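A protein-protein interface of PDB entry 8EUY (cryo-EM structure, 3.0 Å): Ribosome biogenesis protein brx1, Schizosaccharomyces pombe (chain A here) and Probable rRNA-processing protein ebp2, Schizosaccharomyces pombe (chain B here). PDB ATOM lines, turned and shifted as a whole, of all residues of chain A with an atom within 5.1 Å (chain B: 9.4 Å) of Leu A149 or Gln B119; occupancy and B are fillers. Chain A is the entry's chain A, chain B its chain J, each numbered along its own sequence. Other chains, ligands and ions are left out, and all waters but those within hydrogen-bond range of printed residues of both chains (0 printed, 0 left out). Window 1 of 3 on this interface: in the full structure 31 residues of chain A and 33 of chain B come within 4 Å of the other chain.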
ATOM      1  N   ARG A 146      23.607   0.955   7.259  1.00  0.00           N
ATOM      2  CA  ARG A 146      23.547  -0.095   6.249  1.00  0.00           C
ATOM      3  C   ARG A 146      24.126  -1.386   6.810  1.00  0.00           C
ATOM      4  O   ARG A 146      25.293  -1.403   7.220  1.00  0.00           O
ATOM      5  CB  ARG A 146      24.306   0.330   4.997  1.00  0.00           C
ATOM      6  CG  ARG A 146      23.776   1.595   4.347  1.00  0.00           C
ATOM      7  CD  ARG A 146      24.487   1.875   3.034  1.00  0.00           C
ATOM      8  NE  ARG A 146      24.192   0.861   2.029  1.00  0.00           N
ATOM      9  CZ  ARG A 146      25.111   0.226   1.312  1.00  0.00           C
ATOM     10  NH1 ARG A 146      26.401   0.473   1.468  1.00  0.00           N
ATOM     11  NH2 ARG A 146      24.724  -0.679   0.418  1.00  0.00           N
ATOM     12  N   PRO A 147      23.364  -2.477   6.850  1.00  0.00           N
ATOM     13  CA  PRO A 147      23.900  -3.733   7.387  1.00  0.00           C
ATOM     14  C   PRO A 147      24.593  -4.569   6.324  1.00  0.00           C
ATOM     15  O   PRO A 147      24.707  -4.153   5.167  1.00  0.00           O
ATOM     16  CB  PRO A 147      22.650  -4.435   7.923  1.00  0.00           C
ATOM     17  CG  PRO A 147      21.560  -3.975   7.004  1.00  0.00           C
ATOM     18  CD  PRO A 147      21.937  -2.594   6.502  1.00  0.00           C
ATOM     19  N   ILE A 148      25.063  -5.751   6.712  1.00  0.00           N
ATOM     20  CA  ILE A 148      25.658  -6.711   5.790  1.00  0.00           C
ATOM     21  C   ILE A 148      24.769  -7.945   5.774  1.00  0.00           C
ATOM     22  O   ILE A 148      24.521  -8.553   6.823  1.00  0.00           O
ATOM     23  CB  ILE A 148      27.097  -7.075   6.187  1.00  0.00           C
ATOM     24  CG1 ILE A 148      27.910  -5.806   6.447  1.00  0.00           C
ATOM     25  CG2 ILE A 148      27.748  -7.920   5.104  1.00  0.00           C
ATOM     26  CD1 ILE A 148      29.144  -6.034   7.294  1.00  0.00           C
ATOM     27  N   LEU A 149      24.287  -8.312   4.589  1.00  0.00           N
ATOM     28  CA  LEU A 149      23.375  -9.440   4.434  1.00  0.00           C
ATOM     29  C   LEU A 149      24.187 -10.691   4.121  1.00  0.00           C
ATOM     30  O   LEU A 149      24.829 -10.777   3.070  1.00  0.00           O
ATOM     31  CB  LEU A 149      22.354  -9.159   3.334  1.00  0.00           C
ATOM     32  CG  LEU A 149      21.525  -7.880   3.464  1.00  0.00           C
ATOM     33  CD1 LEU A 149      20.373  -7.889   2.472  1.00  0.00           C
ATOM     34  CD2 LEU A 149      21.008  -7.708   4.884  1.00  0.00           C
ATOM     35  N   SER A 150      24.157 -11.659   5.032  1.00  0.00           N
ATOM     36  CA  SER A 150      24.843 -12.932   4.850  1.00  0.00           C
ATOM     37  C   SER A 150      23.810 -14.006   4.528  1.00  0.00           C
ATOM     38  O   SER A 150      22.866 -14.216   5.297  1.00  0.00           O
ATOM     39  CB  SER A 150      25.642 -13.305   6.098  1.00  0.00           C
ATOM     40  OG  SER A 150      24.852 -13.178   7.267  1.00  0.00           O
ATOM     41  N   PHE A 151      23.993 -14.681   3.397  1.00  0.00           N
ATOM     42  CA  PHE A 151      23.057 -15.687   2.917  1.00  0.00           C
ATOM     43  C   PHE A 151      23.726 -17.055   2.931  1.00  0.00           C
ATOM     44  O   PHE A 151      24.871 -17.196   2.489  1.00  0.00           O
ATOM     45  CB  PHE A 151      22.569 -15.350   1.506  1.00  0.00           C
ATOM     46  CG  PHE A 151      21.714 -14.119   1.442  1.00  0.00           C
ATOM     47  CD1 PHE A 151      20.366 -14.177   1.751  1.00  0.00           C
ATOM     48  CD2 PHE A 151      22.259 -12.899   1.076  1.00  0.00           C
ATOM     49  CE1 PHE A 151      19.576 -13.044   1.692  1.00  0.00           C
ATOM     50  CE2 PHE A 151      21.474 -11.763   1.017  1.00  0.00           C
ATOM     51  CZ  PHE A 151      20.132 -11.836   1.325  1.00  0.00           C
ATOM     52  N   LEU A 168      15.154 -11.107  -1.041  1.00  0.00           N
ATOM     53  CA  LEU A 168      15.475 -10.585   0.285  1.00  0.00           C
ATOM     54  C   LEU A 168      16.663  -9.634   0.232  1.00  0.00           C
ATOM     55  O   LEU A 168      16.680  -8.614   0.930  1.00  0.00           O
ATOM     56  CB  LEU A 168      15.752 -11.736   1.250  1.00  0.00           C
ATOM     57  CG  LEU A 168      14.532 -12.519   1.737  1.00  0.00           C
ATOM     58  CD1 LEU A 168      14.962 -13.722   2.559  1.00  0.00           C
ATOM     59  CD2 LEU A 168      13.608 -11.619   2.541  1.00  0.00           C
ATOM     60  N   GLN A 169      17.670  -9.957  -0.584  1.00  0.00           N
ATOM     61  CA  GLN A 169      18.824  -9.074  -0.725  1.00  0.00           C
ATOM     62  C   GLN A 169      18.415  -7.722  -1.295  1.00  0.00           C
ATOM     63  O   GLN A 169      18.874  -6.675  -0.824  1.00  0.00           O
ATOM     64  CB  GLN A 169      19.880  -9.737  -1.610  1.00  0.00           C
ATOM     65  CG  GLN A 169      20.753  -8.762  -2.383  1.00  0.00           C
ATOM     66  CD  GLN A 169      21.294  -9.359  -3.667  1.00  0.00           C
ATOM     67  OE1 GLN A 169      21.597 -10.550  -3.732  1.00  0.00           O
ATOM     68  NE2 GLN A 169      21.414  -8.532  -4.700  1.00  0.00           N
ATOM     69  N   PHE A 172      15.795  -6.159   1.844  1.00  0.00           N
ATOM     70  CA  PHE A 172      16.378  -5.875   3.152  1.00  0.00           C
ATOM     71  C   PHE A 172      17.559  -4.918   3.044  1.00  0.00           C
ATOM     72  O   PHE A 172      17.698  -3.998   3.860  1.00  0.00           O
ATOM     73  CB  PHE A 172      16.807  -7.175   3.830  1.00  0.00           C
ATOM     74  CG  PHE A 172      15.788  -7.727   4.784  1.00  0.00           C
ATOM     75  CD1 PHE A 172      15.489  -7.057   5.958  1.00  0.00           C
ATOM     76  CD2 PHE A 172      15.134  -8.915   4.509  1.00  0.00           C
ATOM     77  CE1 PHE A 172      14.553  -7.562   6.842  1.00  0.00           C
ATOM     78  CE2 PHE A 172      14.198  -9.425   5.387  1.00  0.00           C
ATOM     79  CZ  PHE A 172      13.907  -8.748   6.555  1.00  0.00           C
ATOM     80  N   GLY A 173      18.422  -5.120   2.053  1.00  0.00           N
ATOM     81  CA  GLY A 173      19.574  -4.259   1.874  1.00  0.00           C
ATOM     82  C   GLY A 173      19.205  -2.833   1.525  1.00  0.00           C
ATOM     83  O   GLY A 173      18.485  -2.592   0.551  1.00  0.00           O
ATOM     84  N   CYS A 189      22.791  -8.968   9.161  1.00  0.00           N
ATOM     85  CA  CYS A 189      21.638  -9.854   9.077  1.00  0.00           C
ATOM     86  C   CYS A 189      22.083 -11.209   8.545  1.00  0.00           C
ATOM     87  O   CYS A 189      22.732 -11.287   7.497  1.00  0.00           O
ATOM     88  CB  CYS A 189      20.556  -9.259   8.176  1.00  0.00           C
ATOM     89  SG  CYS A 189      19.835  -7.719   8.785  1.00  0.00           S
ATOM     90  N   ILE B 113      27.826  -5.062  -9.870  1.00  0.00           N
ATOM     91  CA  ILE B 113      27.563  -4.162  -8.753  1.00  0.00           C
ATOM     92  C   ILE B 113      28.513  -4.481  -7.609  1.00  0.00           C
ATOM     93  O   ILE B 113      28.720  -5.649  -7.257  1.00  0.00           O
ATOM     94  CB  ILE B 113      26.096  -4.270  -8.313  1.00  0.00           C
ATOM     95  N   SER B 114      29.099  -3.438  -7.028  1.00  0.00           N
ATOM     96  CA  SER B 114      30.060  -3.619  -5.953  1.00  0.00           C
ATOM     97  C   SER B 114      29.390  -4.210  -4.718  1.00  0.00           C
ATOM     98  O   SER B 114      28.209  -3.977  -4.450  1.00  0.00           O
ATOM     99  CB  SER B 114      30.721  -2.287  -5.600  1.00  0.00           C
ATOM    100  N   PHE B 115      30.164  -4.996  -3.966  1.00  0.00           N
ATOM    101  CA  PHE B 115      29.645  -5.584  -2.736  1.00  0.00           C
ATOM    102  C   PHE B 115      29.314  -4.517  -1.702  1.00  0.00           C
ATOM    103  O   PHE B 115      28.385  -4.694  -0.906  1.00  0.00           O
ATOM    104  CB  PHE B 115      30.653  -6.583  -2.165  1.00  0.00           C
ATOM    105  N   VAL B 116      30.063  -3.413  -1.691  1.00  0.00           N
ATOM    106  CA  VAL B 116      29.758  -2.318  -0.774  1.00  0.00           C
ATOM    107  C   VAL B 116      28.403  -1.707  -1.107  1.00  0.00           C
ATOM    108  O   VAL B 116      27.598  -1.420  -0.212  1.00  0.00           O
ATOM    109  CB  VAL B 116      30.879  -1.264  -0.808  1.00  0.00           C
ATOM    110  N   GLU B 117      28.133  -1.491  -2.397  1.00  0.00           N
ATOM    111  CA  GLU B 117      26.842  -0.945  -2.802  1.00  0.00           C
ATOM    112  C   GLU B 117      25.707  -1.913  -2.491  1.00  0.00           C
ATOM    113  O   GLU B 117      24.648  -1.499  -2.004  1.00  0.00           O
ATOM    114  CB  GLU B 117      26.862  -0.602  -4.291  1.00  0.00           C
ATOM    115  N   ASN B 118      25.909  -3.203  -2.763  1.00  0.00           N
ATOM    116  CA  ASN B 118      24.872  -4.192  -2.494  1.00  0.00           C
ATOM    117  C   ASN B 118      24.745  -4.503  -1.009  1.00  0.00           C
ATOM    118  O   ASN B 118      23.651  -4.848  -0.547  1.00  0.00           O
ATOM    119  CB  ASN B 118      25.155  -5.477  -3.274  1.00  0.00           C
ATOM    120  N   GLN B 119      25.841  -4.387  -0.255  1.00  0.00           N
ATOM    121  CA  GLN B 119      25.860  -4.682   1.180  1.00  0.00           C
ATOM    122  C   GLN B 119      25.372  -6.101   1.462  1.00  0.00           C
ATOM    123  O   GLN B 119      24.685  -6.358   2.452  1.00  0.00           O
ATOM    124  CB  GLN B 119      25.039  -3.657   1.967  1.00  0.00           C
ATOM    125  N   ALA B 120      25.738  -7.033   0.584  1.00  0.00           N
ATOM    126  CA  ALA B 120      25.363  -8.433   0.710  1.00  0.00           C
ATOM    127  C   ALA B 120      26.614  -9.298   0.692  1.00  0.00           C
ATOM    128  O   ALA B 120      27.568  -9.012  -0.037  1.00  0.00           O
ATOM    129  CB  ALA B 120      24.414  -8.858  -0.414  1.00  0.00           C
ATOM    130  N   VAL B 121      26.605 -10.358   1.498  1.00  0.00           N
ATOM    131  CA  VAL B 121      27.744 -11.256   1.636  1.00  0.00           C
ATOM    132  C   VAL B 121      27.275 -12.679   1.371  1.00  0.00           C
ATOM    133  O   VAL B 121      26.234 -13.101   1.886  1.00  0.00           O
ATOM    134  CB  VAL B 121      28.390 -11.150   3.031  1.00  0.00           C
ATOM    135  N   THR B 122      28.040 -13.412   0.567  1.00  0.00           N
ATOM    136  CA  THR B 122      27.757 -14.802   0.223  1.00  0.00           C
ATOM    137  C   THR B 122      29.017 -15.645   0.371  1.00  0.00           C
ATOM    138  O   THR B 122      29.389 -16.419  -0.514  1.00  0.00           O
ATOM    139  CB  THR B 122      27.195 -14.916  -1.191  1.00  0.00           C
ATOM    140  N   THR B 123      29.697 -15.487   1.505  1.00  0.00           N
ATOM    141  CA  THR B 123      30.952 -16.189   1.737  1.00  0.00           C
ATOM    142  C   THR B 123      30.736 -17.698   1.760  1.00  0.00           C
ATOM    143  O   THR B 123      29.712 -18.191   2.243  1.00  0.00           O
ATOM    144  CB  THR B 123      31.581 -15.733   3.055  1.00  0.00           C
ATOM    145  N   GLN B 145      29.645 -18.146  10.233  1.00  0.00           N
ATOM    146  CA  GLN B 145      29.407 -17.603   8.899  1.00  0.00           C
ATOM    147  C   GLN B 145      29.267 -16.086   8.942  1.00  0.00           C
ATOM    148  O   GLN B 145      29.762 -15.387   8.051  1.00  0.00           O
ATOM    149  CB  GLN B 145      28.161 -18.242   8.286  1.00  0.00           C
ATOM    150  N   GLY B 146      28.594 -15.563   9.969  1.00  0.00           N
ATOM    151  CA  GLY B 146      28.451 -14.123  10.092  1.00  0.00           C
ATOM    152  C   GLY B 146      29.771 -13.420  10.348  1.00  0.00           C
ATOM    153  O   GLY B 146      30.018 -12.334   9.819  1.00  0.00           O
ATOM    154  N   SER B 149      31.596 -13.405   7.086  1.00  0.00           N
ATOM    155  CA  SER B 149      30.960 -12.445   6.190  1.00  0.00           C
ATOM    156  C   SER B 149      31.276 -11.012   6.600  1.00  0.00           C
ATOM    157  O   SER B 149      31.529 -10.154   5.746  1.00  0.00           O
ATOM    158  CB  SER B 149      29.450 -12.676   6.164  1.00  0.00           C
ATOM    159  N   VAL B 150      31.262 -10.732   7.906  1.00  0.00           N
ATOM    160  CA  VAL B 150      31.561  -9.385   8.384  1.00  0.00           C
ATOM    161  C   VAL B 150      33.004  -9.013   8.071  1.00  0.00           C
ATOM    162  O   VAL B 150      33.292  -7.891   7.638  1.00  0.00           O
ATOM    163  CB  VAL B 150      31.261  -9.273   9.891  1.00  0.00           C
ATOM    164  N   ALA B 153      33.341  -8.354   4.294  1.00  0.00           N
ATOM    165  CA  ALA B 153      32.747  -7.070   3.934  1.00  0.00           C
ATOM    166  C   ALA B 153      33.584  -5.908   4.450  1.00  0.00           C
ATOM    167  O   ALA B 153      33.738  -4.893   3.760  1.00  0.00           O
ATOM    168  CB  ALA B 153      31.318  -6.984   4.467  1.00  0.00           C
ATOM    169  N   LYS B 156      36.432  -5.534   2.159  1.00  0.00           N
ATOM    170  CA  LYS B 156      35.955  -4.953   0.908  1.00  0.00           C
ATOM    171  C   LYS B 156      35.668  -3.464   1.067  1.00  0.00           C
ATOM    172  O   LYS B 156      35.982  -2.666   0.177  1.00  0.00           O
ATOM    173  CB  LYS B 156      34.707  -5.693   0.427  1.00  0.00           C
ATOM    174  N   LEU B 157      35.065  -3.075   2.194  1.00  0.00           N
ATOM    175  CA  LEU B 157      34.798  -1.662   2.440  1.00  0.00           C
ATOM    176  C   LEU B 157      36.093  -0.867   2.557  1.00  0.00           C
ATOM    177  O   LEU B 157      36.190   0.255   2.049  1.00  0.00           O
ATOM    178  CB  LEU B 157      33.952  -1.500   3.702  1.00  0.00           C
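O of Val B116 lies within hydrogen-bond range of NH1 of Arg A146, at 2.8 Å. The backbone carbonyl oxygen (O) of Glu B117 sits at hydrogen-bond distance from the guanidinium group (NH2) of Arg A146. O of Gln B119 sits at hydrogen-bond distance from N of Leu A149, 2.9 Å away. The backbone NH (N) of Val B121 is in hydrogen-bond range of the backbone carbonyl oxygen (O) of Leu A149 (2.4 Å). The backbone carbonyl oxygen (O) of Val B121 sits at hydrogen-bond distance from the backbone NH (N) of Phe A151. O of Pro A147 lies close to O of Gln B119 (3.5 Å).
Of the printed residues of chain B, Pro A147 touches Gln B119 (3.3 Å). Printed residues of chain A within 4 Å of Glu B117: Arg A146. Gln B119 touches just these residues of chain A: Arg A146 (3.4 Å), Pro A147 (3.3 Å), Ile A148 (3.5 Å) and Leu A149 (2.9 Å). The nearest residue of chain B that does not touch Leu A149 is Thr B122 (4.8 Å). The nearest printed residue of chain B that does not touch Phe A151 is Ala B120 (4.4 Å).
O of Ile A148 lies within hydrogen-bond range of N of Cys A189, at 2.9 Å. O of Cys A189 lies within hydrogen-bond range of OG of Ser A150 (2.9 Å).
Hydrophobic or aromatic side chains of chain A within 4 Å of the printed part of chain B: Ile A148 and Leu A149. Along chain A the printed residues that touch a printed residue of chain B span positions 146 to 151. Of the 18 printed residues of chain B, 7 touch a printed residue of chain A. Printed residues of chain B that touch a printed residue of chain A: Val B116, Glu B117, Gln B119, Ala B120, Val B121, Ser B149 and Ala B153. Hydrophobic or aromatic side chains of chain B within 4 Å of the printed part of chain A: Ala B120, Val B121 and Ala B153. Along chain B the printed residues that touch a printed residue of chain A span positions 116 to 153. Among the printed residues, 13 pairs touch across the chains.
Among the printed residues, pairs that only touch across the chains: Ser A150 with Val B121, Leu A149 with Ala B120, Arg A146 with Gln B119, Ile A148 with Gln B119, Ile A148 with Ala B153, Ser A150 with Ser B149 and Ile A148 with Val B121.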
